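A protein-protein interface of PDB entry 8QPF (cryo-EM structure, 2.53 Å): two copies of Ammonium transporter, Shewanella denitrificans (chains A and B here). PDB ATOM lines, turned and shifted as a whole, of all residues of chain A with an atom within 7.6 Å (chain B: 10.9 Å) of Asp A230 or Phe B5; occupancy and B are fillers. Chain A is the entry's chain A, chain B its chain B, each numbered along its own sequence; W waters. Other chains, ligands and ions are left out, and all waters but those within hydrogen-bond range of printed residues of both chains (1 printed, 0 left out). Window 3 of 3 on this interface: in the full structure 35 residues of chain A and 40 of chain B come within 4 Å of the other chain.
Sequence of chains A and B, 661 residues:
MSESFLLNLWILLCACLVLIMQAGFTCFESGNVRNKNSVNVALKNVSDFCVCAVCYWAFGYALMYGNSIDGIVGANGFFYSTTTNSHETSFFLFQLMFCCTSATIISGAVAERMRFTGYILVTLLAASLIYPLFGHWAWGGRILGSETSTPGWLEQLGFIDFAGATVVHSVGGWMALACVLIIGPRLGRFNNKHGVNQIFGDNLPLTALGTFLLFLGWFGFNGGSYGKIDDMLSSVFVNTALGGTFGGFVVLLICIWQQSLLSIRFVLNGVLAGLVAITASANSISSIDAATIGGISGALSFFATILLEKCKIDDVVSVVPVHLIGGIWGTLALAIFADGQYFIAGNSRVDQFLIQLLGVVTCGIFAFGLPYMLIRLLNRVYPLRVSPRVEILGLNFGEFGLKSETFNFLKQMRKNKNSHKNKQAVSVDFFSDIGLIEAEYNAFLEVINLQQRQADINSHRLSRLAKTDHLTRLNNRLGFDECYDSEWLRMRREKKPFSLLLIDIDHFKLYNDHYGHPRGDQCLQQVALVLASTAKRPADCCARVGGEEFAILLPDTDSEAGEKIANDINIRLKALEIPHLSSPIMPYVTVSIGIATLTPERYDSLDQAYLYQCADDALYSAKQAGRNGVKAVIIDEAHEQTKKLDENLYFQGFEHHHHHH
CD1 of Leu B6 touches CD1 of Leu A6, 3.9 Å away. CD1 of Leu B9 touches CD1 of Leu A6, at 3.7 Å. Ile A229 touches Phe B5. Ile A229 touches Leu B9. Asp A230 touches Phe B5. Asp A231 touches Phe B5 (N to CE1, 3.7 Å). Leu A233 touches Leu B9 (CD2 to CD2, 3.7 Å). CD2 of Leu B12 touches OG of Ser A234 (3.5 Å). Ser A234 touches Thr B89 (CB to CB, 3.8 Å).
The side-chain hydroxyl (OG) of Ser A234 sits close to the side-chain hydroxyl (OG) of Ser B90 (2.3 Å).
Asp A230 touches just one residue of chain B: Phe B5. Phe B5 touches just these residues of chain A: Ile A229 (3.8 Å), Asp A230 (3.6 Å) and Asp A231 (3.7 Å). No residue of chain B comes within 4 Å of Lys A228. Of chain B, only Phe B5 (3.8 Å) and Leu B9 (3.7 Å) come within 4 Å of Ile A229. Leu A233 touches just one residue of chain B: Leu B9. No residue of chain A comes within 4 Å of Ser B4. Of the printed residues of chain B, Leu A6 touches Leu B6 (3.9 Å) and Leu B9 (3.7 Å). Of the printed residues of chain A, Ser B90 touches Ser A234. Printed residues of chain A within 4 Å of Leu B12: Ser A234 (3.5 Å). Printed residues of chain A within 4 Å of Leu B6: Leu A6. Of the printed residues of chain A, Thr B89 touches Ser A234 (3.8 Å). Tyr A226 touches none of the printed residues of chain B. Thr B82 touches none of the printed residues of chain A. The nearest residue of chain A that does not touch Phe B5 is Leu A6 (5.1 Å).
Of the 24 printed residues of chain B, 6 touch a printed residue of chain A. Among the printed residues, no Asp or Glu carboxylate lies within 4 Å of a Lys or Arg side-chain nitrogen of the other chain.
Water W1 lies within hydrogen-bond range of O of Asp A231 (2.8 Å), OG of Ser A235 (2.9 Å), OG1 of Thr B89 (3.4 Å) and SD of Met A232 (3.8 Å).
Leu A6 touches its own counterpart, Leu B6.
OD1 of Asp A230 sits close to OH of Tyr A226, at 3.2 Å.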
ATOM      1  N   GLU A   3      24.342  21.610  -8.349  1.00  0.00           N
ATOM      2  CA  GLU A   3      22.883  21.607  -8.325  1.00  0.00           C
ATOM      3  C   GLU A   3      22.319  22.989  -8.634  1.00  0.00           C
ATOM      4  O   GLU A   3      21.286  23.110  -9.306  1.00  0.00           O
ATOM      5  CB  GLU A   3      22.387  21.124  -6.963  1.00  0.00           C
ATOM      6  CG  GLU A   3      22.925  19.768  -6.543  1.00  0.00           C
ATOM      7  CD  GLU A   3      22.315  19.282  -5.243  1.00  0.00           C
ATOM      8  OE1 GLU A   3      21.458  19.998  -4.684  1.00  0.00           O
ATOM      9  OE2 GLU A   3      22.693  18.185  -4.779  1.00  0.00           O
ATOM     10  N   LEU A   6      22.393  23.878 -12.474  1.00  0.00           N
ATOM     11  CA  LEU A   6      21.397  23.135 -13.239  1.00  0.00           C
ATOM     12  C   LEU A   6      19.990  23.633 -12.921  1.00  0.00           C
ATOM     13  O   LEU A   6      19.142  23.737 -13.818  1.00  0.00           O
ATOM     14  CB  LEU A   6      21.535  21.641 -12.942  1.00  0.00           C
ATOM     15  CG  LEU A   6      20.656  20.594 -13.632  1.00  0.00           C
ATOM     16  CD1 LEU A   6      20.410  20.937 -15.101  1.00  0.00           C
ATOM     17  CD2 LEU A   6      21.271  19.211 -13.498  1.00  0.00           C
ATOM     18  N   TYR A 226       7.894  24.045 -10.031  1.00  0.00           N
ATOM     19  CA  TYR A 226       8.288  22.935  -9.166  1.00  0.00           C
ATOM     20  C   TYR A 226       9.328  23.357  -8.132  1.00  0.00           C
ATOM     21  O   TYR A 226       9.261  22.940  -6.970  1.00  0.00           O
ATOM     22  CB  TYR A 226       8.808  21.777 -10.010  1.00  0.00           C
ATOM     23  CG  TYR A 226       8.856  20.474  -9.263  1.00  0.00           C
ATOM     24  CD1 TYR A 226       7.707  19.934  -8.700  1.00  0.00           C
ATOM     25  CD2 TYR A 226      10.048  19.787  -9.111  1.00  0.00           C
ATOM     26  CE1 TYR A 226       7.747  18.740  -8.009  1.00  0.00           C
ATOM     27  CE2 TYR A 226      10.099  18.601  -8.424  1.00  0.00           C
ATOM     28  CZ  TYR A 226       8.948  18.080  -7.876  1.00  0.00           C
ATOM     29  OH  TYR A 226       9.004  16.892  -7.190  1.00  0.00           O
ATOM     30  N   LYS A 228      12.474  22.671  -7.642  1.00  0.00           N
ATOM     31  CA  LYS A 228      13.600  21.798  -7.336  1.00  0.00           C
ATOM     32  C   LYS A 228      13.788  20.851  -8.512  1.00  0.00           C
ATOM     33  O   LYS A 228      13.036  20.886  -9.489  1.00  0.00           O
ATOM     34  CB  LYS A 228      13.382  21.034  -6.027  1.00  0.00           C
ATOM     35  CG  LYS A 228      11.970  20.516  -5.833  1.00  0.00           C
ATOM     36  CD  LYS A 228      11.841  19.755  -4.527  1.00  0.00           C
ATOM     37  CE  LYS A 228      10.432  19.229  -4.330  1.00  0.00           C
ATOM     38  NZ  LYS A 228      10.340  18.335  -3.144  1.00  0.00           N
ATOM     39  N   ILE A 229      14.820  20.015  -8.426  1.00  0.00           N
ATOM     40  CA  ILE A 229      15.126  19.032  -9.460  1.00  0.00           C
ATOM     41  C   ILE A 229      15.309  17.684  -8.777  1.00  0.00           C
ATOM     42  O   ILE A 229      16.263  17.496  -8.012  1.00  0.00           O
ATOM     43  CB  ILE A 229      16.375  19.403 -10.273  1.00  0.00           C
ATOM     44  CG1 ILE A 229      16.152  20.708 -11.043  1.00  0.00           C
ATOM     45  CG2 ILE A 229      16.732  18.276 -11.233  1.00  0.00           C
ATOM     46  CD1 ILE A 229      17.277  21.085 -11.961  1.00  0.00           C
ATOM     47  N   ASP A 230      14.396  16.758  -9.040  1.00  0.00           N
ATOM     48  CA  ASP A 230      14.550  15.364  -8.640  1.00  0.00           C
ATOM     49  C   ASP A 230      13.806  14.508  -9.661  1.00  0.00           C
ATOM     50  O   ASP A 230      13.509  14.965 -10.769  1.00  0.00           O
ATOM     51  CB  ASP A 230      14.086  15.145  -7.186  1.00  0.00           C
ATOM     52  CG  ASP A 230      12.781  15.840  -6.870  1.00  0.00           C
ATOM     53  OD1 ASP A 230      12.078  16.252  -7.808  1.00  0.00           O
ATOM     54  OD2 ASP A 230      12.456  15.972  -5.672  1.00  0.00           O
ATOM     55  N   ASP A 231      13.510  13.262  -9.296  1.00  0.00           N
ATOM     56  CA  ASP A 231      12.871  12.335 -10.220  1.00  0.00           C
ATOM     57  C   ASP A 231      11.361  12.518 -10.320  1.00  0.00           C
ATOM     58  O   ASP A 231      10.737  11.877 -11.171  1.00  0.00           O
ATOM     59  CB  ASP A 231      13.182  10.891  -9.815  1.00  0.00           C
ATOM     60  CG  ASP A 231      13.351  10.724  -8.317  1.00  0.00           C
ATOM     61  OD1 ASP A 231      13.055  11.679  -7.568  1.00  0.00           O
ATOM     62  OD2 ASP A 231      13.781   9.634  -7.886  1.00  0.00           O
ATOM     63  N   MET A 232      10.760  13.364  -9.488  1.00  0.00           N
ATOM     64  CA  MET A 232       9.313  13.538  -9.476  1.00  0.00           C
ATOM     65  C   MET A 232       8.832  14.703 -10.334  1.00  0.00           C
ATOM     66  O   MET A 232       7.626  14.970 -10.366  1.00  0.00           O
ATOM     67  CB  MET A 232       8.817  13.718  -8.038  1.00  0.00           C
ATOM     68  CG  MET A 232       8.681  12.424  -7.260  1.00  0.00           C
ATOM     69  SD  MET A 232       7.605  11.235  -8.083  1.00  0.00           S
ATOM     70  CE  MET A 232       5.996  11.803  -7.540  1.00  0.00           C
ATOM     71  N   LEU A 233       9.737  15.405 -11.019  1.00  0.00           N
ATOM     72  CA  LEU A 233       9.331  16.470 -11.934  1.00  0.00           C
ATOM     73  C   LEU A 233       8.690  15.903 -13.199  1.00  0.00           C
ATOM     74  O   LEU A 233       7.841  16.559 -13.826  1.00  0.00           O
ATOM     75  CB  LEU A 233      10.547  17.336 -12.263  1.00  0.00           C
ATOM     76  CG  LEU A 233      10.443  18.520 -13.220  1.00  0.00           C
ATOM     77  CD1 LEU A 233       9.304  19.435 -12.834  1.00  0.00           C
ATOM     78  CD2 LEU A 233      11.748  19.273 -13.190  1.00  0.00           C
ATOM     79  N   SER A 234       9.076  14.682 -13.572  1.00  0.00           N
ATOM     80  CA  SER A 234       8.461  14.005 -14.705  1.00  0.00           C
ATOM     81  C   SER A 234       6.996  13.690 -14.443  1.00  0.00           C
ATOM     82  O   SER A 234       6.189  13.682 -15.378  1.00  0.00           O
ATOM     83  CB  SER A 234       9.234  12.729 -15.018  1.00  0.00           C
ATOM     84  OG  SER A 234      10.351  13.020 -15.830  1.00  0.00           O
ATOM     85  N   SER A 235       6.635  13.444 -13.179  1.00  0.00           N
ATOM     86  CA  SER A 235       5.232  13.273 -12.817  1.00  0.00           C
ATOM     87  C   SER A 235       4.449  14.565 -13.019  1.00  0.00           C
ATOM     88  O   SER A 235       3.288  14.530 -13.441  1.00  0.00           O
ATOM     89  CB  SER A 235       5.116  12.797 -11.370  1.00  0.00           C
ATOM     90  OG  SER A 235       5.674  11.506 -11.214  1.00  0.00           O
ATOM     91  N   VAL A 236       5.075  15.710 -12.732  1.00  0.00           N
ATOM     92  CA  VAL A 236       4.447  17.010 -12.969  1.00  0.00           C
ATOM     93  C   VAL A 236       4.217  17.231 -14.460  1.00  0.00           C
ATOM     94  O   VAL A 236       3.147  17.700 -14.878  1.00  0.00           O
ATOM     95  CB  VAL A 236       5.308  18.131 -12.353  1.00  0.00           C
ATOM     96  CG1 VAL A 236       4.627  19.479 -12.489  1.00  0.00           C
ATOM     97  CG2 VAL A 236       5.614  17.828 -10.899  1.00  0.00           C
ATOM     98  N   SER B   2      22.756  15.021 -10.319  1.00  0.00           N
ATOM     99  CA  SER B   2      23.435  13.811 -10.762  1.00  0.00           C
ATOM    100  C   SER B   2      23.198  13.553 -12.248  1.00  0.00           C
ATOM    101  O   SER B   2      22.685  14.414 -12.963  1.00  0.00           O
ATOM    102  CB  SER B   2      22.973  12.606  -9.940  1.00  0.00           C
ATOM    103  OG  SER B   2      21.785  12.049 -10.473  1.00  0.00           O
ATOM    104  N   GLU B   3      23.589  12.360 -12.703  1.00  0.00           N
ATOM    105  CA  GLU B   3      23.398  11.995 -14.104  1.00  0.00           C
ATOM    106  C   GLU B   3      21.930  11.741 -14.418  1.00  0.00           C
ATOM    107  O   GLU B   3      21.448  12.098 -15.501  1.00  0.00           O
ATOM    108  CB  GLU B   3      24.231  10.758 -14.437  1.00  0.00           C
ATOM    109  CG  GLU B   3      25.713  10.896 -14.138  1.00  0.00           C
ATOM    110  CD  GLU B   3      26.508   9.689 -14.594  1.00  0.00           C
ATOM    111  OE1 GLU B   3      25.901   8.758 -15.163  1.00  0.00           O
ATOM    112  OE2 GLU B   3      27.739   9.670 -14.383  1.00  0.00           O
ATOM    113  N   SER B   4      21.211  11.113 -13.480  1.00  0.00           N
ATOM    114  CA  SER B   4      19.819  10.734 -13.709  1.00  0.00           C
ATOM    115  C   SER B   4      18.916  11.953 -13.824  1.00  0.00           C
ATOM    116  O   SER B   4      18.011  11.983 -14.666  1.00  0.00           O
ATOM    117  CB  SER B   4      19.339   9.819 -12.583  1.00  0.00           C
ATOM    118  OG  SER B   4      19.452  10.462 -11.327  1.00  0.00           O
ATOM    119  N   PHE B   5      19.153  12.970 -12.988  1.00  0.00           N
ATOM    120  CA  PHE B   5      18.342  14.185 -13.035  1.00  0.00           C
ATOM    121  C   PHE B   5      18.554  14.942 -14.339  1.00  0.00           C
ATOM    122  O   PHE B   5      17.591  15.414 -14.954  1.00  0.00           O
ATOM    123  CB  PHE B   5      18.667  15.086 -11.843  1.00  0.00           C
ATOM    124  CG  PHE B   5      18.442  14.440 -10.504  1.00  0.00           C
ATOM    125  CD1 PHE B   5      17.410  13.532 -10.313  1.00  0.00           C
ATOM    126  CD2 PHE B   5      19.264  14.750  -9.432  1.00  0.00           C
ATOM    127  CE1 PHE B   5      17.210  12.939  -9.079  1.00  0.00           C
ATOM    128  CE2 PHE B   5      19.066  14.163  -8.194  1.00  0.00           C
ATOM    129  CZ  PHE B   5      18.038  13.258  -8.019  1.00  0.00           C
ATOM    130  N   LEU B   6      19.810  15.048 -14.784  1.00  0.00           N
ATOM    131  CA  LEU B   6      20.115  15.747 -16.028  1.00  0.00           C
ATOM    132  C   LEU B   6      19.559  14.995 -17.233  1.00  0.00           C
ATOM    133  O   LEU B   6      19.044  15.615 -18.175  1.00  0.00           O
ATOM    134  CB  LEU B   6      21.626  15.940 -16.154  1.00  0.00           C
ATOM    135  CG  LEU B   6      22.175  16.739 -17.339  1.00  0.00           C
ATOM    136  CD1 LEU B   6      21.370  18.015 -17.560  1.00  0.00           C
ATOM    137  CD2 LEU B   6      23.646  17.058 -17.136  1.00  0.00           C
ATOM    138  N   LEU B   7      19.629  13.659 -17.206  1.00  0.00           N
ATOM    139  CA  LEU B   7      19.031  12.856 -18.270  1.00  0.00           C
ATOM    140  C   LEU B   7      17.511  13.002 -18.295  1.00  0.00           C
ATOM    141  O   LEU B   7      16.911  13.094 -19.373  1.00  0.00           O
ATOM    142  CB  LEU B   7      19.432  11.389 -18.106  1.00  0.00           C
ATOM    143  CG  LEU B   7      18.940  10.407 -19.172  1.00  0.00           C
ATOM    144  CD1 LEU B   7      19.314  10.884 -20.566  1.00  0.00           C
ATOM    145  CD2 LEU B   7      19.495   9.019 -18.916  1.00  0.00           C
ATOM    146  N   ASN B   8      16.878  13.047 -17.115  1.00  0.00           N
ATOM    147  CA  ASN B   8      15.431  13.224 -17.036  1.00  0.00           C
ATOM    148  C   ASN B   8      15.002  14.580 -17.583  1.00  0.00           C
ATOM    149  O   ASN B   8      14.015  14.671 -18.324  1.00  0.00           O
ATOM    150  CB  ASN B   8      14.964  13.066 -15.589  1.00  0.00           C
ATOM    151  CG  ASN B   8      14.783  11.619 -15.188  1.00  0.00           C
ATOM    152  OD1 ASN B   8      14.715  10.733 -16.037  1.00  0.00           O
ATOM    153  ND2 ASN B   8      14.709  11.370 -13.887  1.00  0.00           N
ATOM    154  N   LEU B   9      15.743  15.640 -17.241  1.00  0.00           N
ATOM    155  CA  LEU B   9      15.440  16.965 -17.776  1.00  0.00           C
ATOM    156  C   LEU B   9      15.655  17.023 -19.282  1.00  0.00           C
ATOM    157  O   LEU B   9      14.904  17.704 -19.993  1.00  0.00           O
ATOM    158  CB  LEU B   9      16.286  18.031 -17.085  1.00  0.00           C
ATOM    159  CG  LEU B   9      16.078  18.214 -15.587  1.00  0.00           C
ATOM    160  CD1 LEU B   9      17.246  18.971 -15.011  1.00  0.00           C
ATOM    161  CD2 LEU B   9      14.778  18.924 -15.305  1.00  0.00           C
ATOM    162  N   TRP B  10      16.675  16.315 -19.784  1.00  0.00           N
ATOM    163  CA  TRP B  10      16.900  16.254 -21.224  1.00  0.00           C
ATOM    164  C   TRP B  10      15.741  15.575 -21.948  1.00  0.00           C
ATOM    165  O   TRP B  10      15.286  16.065 -22.989  1.00  0.00           O
ATOM    166  CB  TRP B  10      18.216  15.534 -21.522  1.00  0.00           C
ATOM    167  CG  TRP B  10      18.579  15.516 -22.981  1.00  0.00           C
ATOM    168  CD1 TRP B  10      18.697  14.417 -23.780  1.00  0.00           C
ATOM    169  CD2 TRP B  10      18.873  16.648 -23.813  1.00  0.00           C
ATOM    170  NE1 TRP B  10      19.039  14.792 -25.053  1.00  0.00           N
ATOM    171  CE2 TRP B  10      19.156  16.155 -25.101  1.00  0.00           C
ATOM    172  CE3 TRP B  10      18.924  18.029 -23.593  1.00  0.00           C
ATOM    173  CZ2 TRP B  10      19.483  16.993 -26.164  1.00  0.00           C
ATOM    174  CZ3 TRP B  10      19.249  18.857 -24.648  1.00  0.00           C
ATOM    175  CH2 TRP B  10      19.526  18.337 -25.918  1.00  0.00           C
ATOM    176  N   ILE B  11      15.227  14.471 -21.394  1.00  0.00           N
ATOM    177  CA  ILE B  11      14.104  13.779 -22.030  1.00  0.00           C
ATOM    178  C   ILE B  11      12.827  14.621 -21.949  1.00  0.00           C
ATOM    179  O   ILE B  11      12.028  14.644 -22.895  1.00  0.00           O
ATOM    180  CB  ILE B  11      13.918  12.373 -21.421  1.00  0.00           C
ATOM    181  CG1 ILE B  11      15.188  11.543 -21.591  1.00  0.00           C
ATOM    182  CG2 ILE B  11      12.796  11.614 -22.107  1.00  0.00           C
ATOM    183  CD1 ILE B  11      15.650  11.404 -23.020  1.00  0.00           C
ATOM    184  N   LEU B  12      12.634  15.354 -20.844  1.00  0.00           N
ATOM    185  CA  LEU B  12      11.469  16.237 -20.731  1.00  0.00           C
ATOM    186  C   LEU B  12      11.520  17.386 -21.739  1.00  0.00           C
ATOM    187  O   LEU B  12      10.506  17.707 -22.377  1.00  0.00           O
ATOM    188  CB  LEU B  12      11.353  16.780 -19.306  1.00  0.00           C
ATOM    189  CG  LEU B  12      10.937  15.785 -18.218  1.00  0.00           C
ATOM    190  CD1 LEU B  12      10.839  16.471 -16.869  1.00  0.00           C
ATOM    191  CD2 LEU B  12       9.632  15.093 -18.571  1.00  0.00           C
ATOM    192  N   LEU B  13      12.696  18.001 -21.916  1.00  0.00           N
ATOM    193  CA  LEU B  13      12.835  19.066 -22.907  1.00  0.00           C
ATOM    194  C   LEU B  13      12.689  18.531 -24.328  1.00  0.00           C
ATOM    195  O   LEU B  13      12.148  19.213 -25.208  1.00  0.00           O
ATOM    196  CB  LEU B  13      14.179  19.775 -22.733  1.00  0.00           C
ATOM    197  CG  LEU B  13      14.333  20.629 -21.472  1.00  0.00           C
ATOM    198  CD1 LEU B  13      15.797  20.943 -21.211  1.00  0.00           C
ATOM    199  CD2 LEU B  13      13.517  21.905 -21.581  1.00  0.00           C
ATOM    200  N   CYS B  14      13.142  17.298 -24.565  1.00  0.00           N
ATOM    201  CA  CYS B  14      12.970  16.696 -25.882  1.00  0.00           C
ATOM    202  C   CYS B  14      11.504  16.379 -26.169  1.00  0.00           C
ATOM    203  O   CYS B  14      11.046  16.542 -27.305  1.00  0.00           O
ATOM    204  CB  CYS B  14      13.846  15.452 -25.994  1.00  0.00           C
ATOM    205  SG  CYS B  14      15.601  15.844 -26.209  1.00  0.00           S
ATOM    206  N   THR B  82       3.158   6.304 -11.435  1.00  0.00           N
ATOM    207  CA  THR B  82       4.571   6.322 -11.077  1.00  0.00           C
ATOM    208  C   THR B  82       5.076   4.919 -10.746  1.00  0.00           C
ATOM    209  O   THR B  82       4.371   4.109 -10.140  1.00  0.00           O
ATOM    210  CB  THR B  82       4.813   7.270  -9.899  1.00  0.00           C
ATOM    211  OG1 THR B  82       6.145   7.090  -9.400  1.00  0.00           O
ATOM    212  CG2 THR B  82       3.799   7.036  -8.778  1.00  0.00           C
ATOM    213  N   THR B  84       8.955   2.359 -10.098  1.00  0.00           N
ATOM    214  CA  THR B  84      10.234   2.377  -9.393  1.00  0.00           C
ATOM    215  C   THR B  84      11.347   2.950 -10.265  1.00  0.00           C
ATOM    216  O   THR B  84      12.317   3.515  -9.748  1.00  0.00           O
ATOM    217  CB  THR B  84      10.597   0.967  -8.925  1.00  0.00           C
ATOM    218  OG1 THR B  84      10.756   0.110 -10.064  1.00  0.00           O
ATOM    219  CG2 THR B  84       9.504   0.406  -8.030  1.00  0.00           C
ATOM    220  N   ASN B  85      11.233   2.798 -11.583  1.00  0.00           N
ATOM    221  CA  ASN B  85      12.261   3.285 -12.495  1.00  0.00           C
ATOM    222  C   ASN B  85      12.223   4.808 -12.578  1.00  0.00           C
ATOM    223  O   ASN B  85      11.158   5.409 -12.752  1.00  0.00           O
ATOM    224  CB  ASN B  85      12.057   2.663 -13.877  1.00  0.00           C
ATOM    225  CG  ASN B  85      13.298   2.735 -14.753  1.00  0.00           C
ATOM    226  OD1 ASN B  85      14.263   3.434 -14.443  1.00  0.00           O
ATOM    227  ND2 ASN B  85      13.267   2.015 -15.867  1.00  0.00           N
ATOM    228  N   SER B  86      13.398   5.430 -12.452  1.00  0.00           N
ATOM    229  CA  SER B  86      13.467   6.888 -12.389  1.00  0.00           C
ATOM    230  C   SER B  86      13.272   7.526 -13.760  1.00  0.00           C
ATOM    231  O   SER B  86      12.623   8.572 -13.874  1.00  0.00           O
ATOM    232  CB  SER B  86      14.802   7.322 -11.781  1.00  0.00           C
ATOM    233  OG  SER B  86      15.893   6.888 -12.575  1.00  0.00           O
ATOM    234  N   HIS B  87      13.827   6.921 -14.807  1.00  0.00           N
ATOM    235  CA  HIS B  87      13.787   7.501 -16.143  1.00  0.00           C
ATOM    236  C   HIS B  87      12.568   7.087 -16.952  1.00  0.00           C
ATOM    237  O   HIS B  87      12.413   7.555 -18.083  1.00  0.00           O
ATOM    238  CB  HIS B  87      15.043   7.116 -16.932  1.00  0.00           C
ATOM    239  CG  HIS B  87      16.323   7.385 -16.207  1.00  0.00           C
ATOM    240  ND1 HIS B  87      16.984   6.416 -15.484  1.00  0.00           N
ATOM    241  CD2 HIS B  87      17.071   8.508 -16.106  1.00  0.00           C
ATOM    242  CE1 HIS B  87      18.081   6.934 -14.961  1.00  0.00           C
ATOM    243  NE2 HIS B  87      18.158   8.200 -15.326  1.00  0.00           N
ATOM    244  N   GLU B  88      11.704   6.226 -16.416  1.00  0.00           N
ATOM    245  CA  GLU B  88      10.650   5.638 -17.232  1.00  0.00           C
ATOM    246  C   GLU B  88       9.450   6.574 -17.404  1.00  0.00           C
ATOM    247  O   GLU B  88       8.731   6.459 -18.400  1.00  0.00           O
ATOM    248  CB  GLU B  88      10.275   4.270 -16.626  1.00  0.00           C
ATOM    249  CG  GLU B  88       8.842   3.770 -16.754  1.00  0.00           C
ATOM    250  CD  GLU B  88       8.712   2.278 -16.552  1.00  0.00           C
ATOM    251  OE1 GLU B  88       8.762   1.832 -15.386  1.00  0.00           O
ATOM    252  OE2 GLU B  88       8.551   1.554 -17.557  1.00  0.00           O
ATOM    253  N   THR B  89       9.261   7.544 -16.507  1.00  0.00           N
ATOM    254  CA  THR B  89       8.155   8.492 -16.655  1.00  0.00           C
ATOM    255  C   THR B  89       8.414   9.485 -17.788  1.00  0.00           C
ATOM    256  O   THR B  89       7.527   9.755 -18.614  1.00  0.00           O
ATOM    257  CB  THR B  89       7.928   9.221 -15.331  1.00  0.00           C
ATOM    258  OG1 THR B  89       8.003   8.281 -14.254  1.00  0.00           O
ATOM    259  CG2 THR B  89       6.569   9.873 -15.303  1.00  0.00           C
ATOM    260  N   SER B  90       9.635  10.032 -17.847  1.00  0.00           N
ATOM    261  CA  SER B  90      10.024  10.895 -18.959  1.00  0.00           C
ATOM    262  C   SER B  90      10.052  10.118 -20.267  1.00  0.00           C
ATOM    263  O   SER B  90       9.685  10.646 -21.325  1.00  0.00           O
ATOM    264  CB  SER B  90      11.393  11.515 -18.691  1.00  0.00           C
ATOM    265  OG  SER B  90      11.558  11.838 -17.328  1.00  0.00           O
ATOM    266  N   LEU B 144      13.958   2.951 -21.177  1.00  0.00           N
ATOM    267  CA  LEU B 144      15.028   3.793 -20.654  1.00  0.00           C
ATOM    268  C   LEU B 144      15.208   3.555 -19.159  1.00  0.00           C
ATOM    269  O   LEU B 144      14.298   3.818 -18.365  1.00  0.00           O
ATOM    270  CB  LEU B 144      14.716   5.261 -20.927  1.00  0.00           C
ATOM    271  CG  LEU B 144      15.772   6.297 -20.545  1.00  0.00           C
ATOM    272  CD1 LEU B 144      17.043   6.101 -21.356  1.00  0.00           C
ATOM    273  CD2 LEU B 144      15.227   7.704 -20.726  1.00  0.00           C
ATOM    274  N   LYS B 228      21.102   8.735 -23.877  1.00  0.00           N
ATOM    275  CA  LYS B 228      22.168   8.960 -22.911  1.00  0.00           C
ATOM    276  C   LYS B 228      22.688  10.377 -23.100  1.00  0.00           C
ATOM    277  O   LYS B 228      22.206  11.130 -23.951  1.00  0.00           O
ATOM    278  CB  LYS B 228      23.292   7.931 -23.061  1.00  0.00           C
ATOM    279  CG  LYS B 228      23.667   7.621 -24.497  1.00  0.00           C
ATOM    280  CD  LYS B 228      24.809   6.626 -24.562  1.00  0.00           C
ATOM    281  CE  LYS B 228      25.205   6.336 -25.997  1.00  0.00           C
ATOM    282  NZ  LYS B 228      26.434   5.499 -26.070  1.00  0.00           N
ATOM    283  N   ILE B 229      23.665  10.752 -22.279  1.00  0.00           N
ATOM    284  CA  ILE B 229      24.303  12.061 -22.358  1.00  0.00           C
ATOM    285  C   ILE B 229      25.810  11.844 -22.378  1.00  0.00           C
ATOM    286  O   ILE B 229      26.381  11.346 -21.400  1.00  0.00           O
ATOM    287  CB  ILE B 229      23.902  12.983 -21.196  1.00  0.00           C
ATOM    288  CG1 ILE B 229      22.403  13.292 -21.241  1.00  0.00           C
ATOM    289  CG2 ILE B 229      24.716  14.269 -21.240  1.00  0.00           C
ATOM    290  CD1 ILE B 229      21.944  14.292 -20.217  1.00  0.00           C
HETATM  291  O   HOH W   1       8.310  10.516 -11.714  1.00  0.00           O
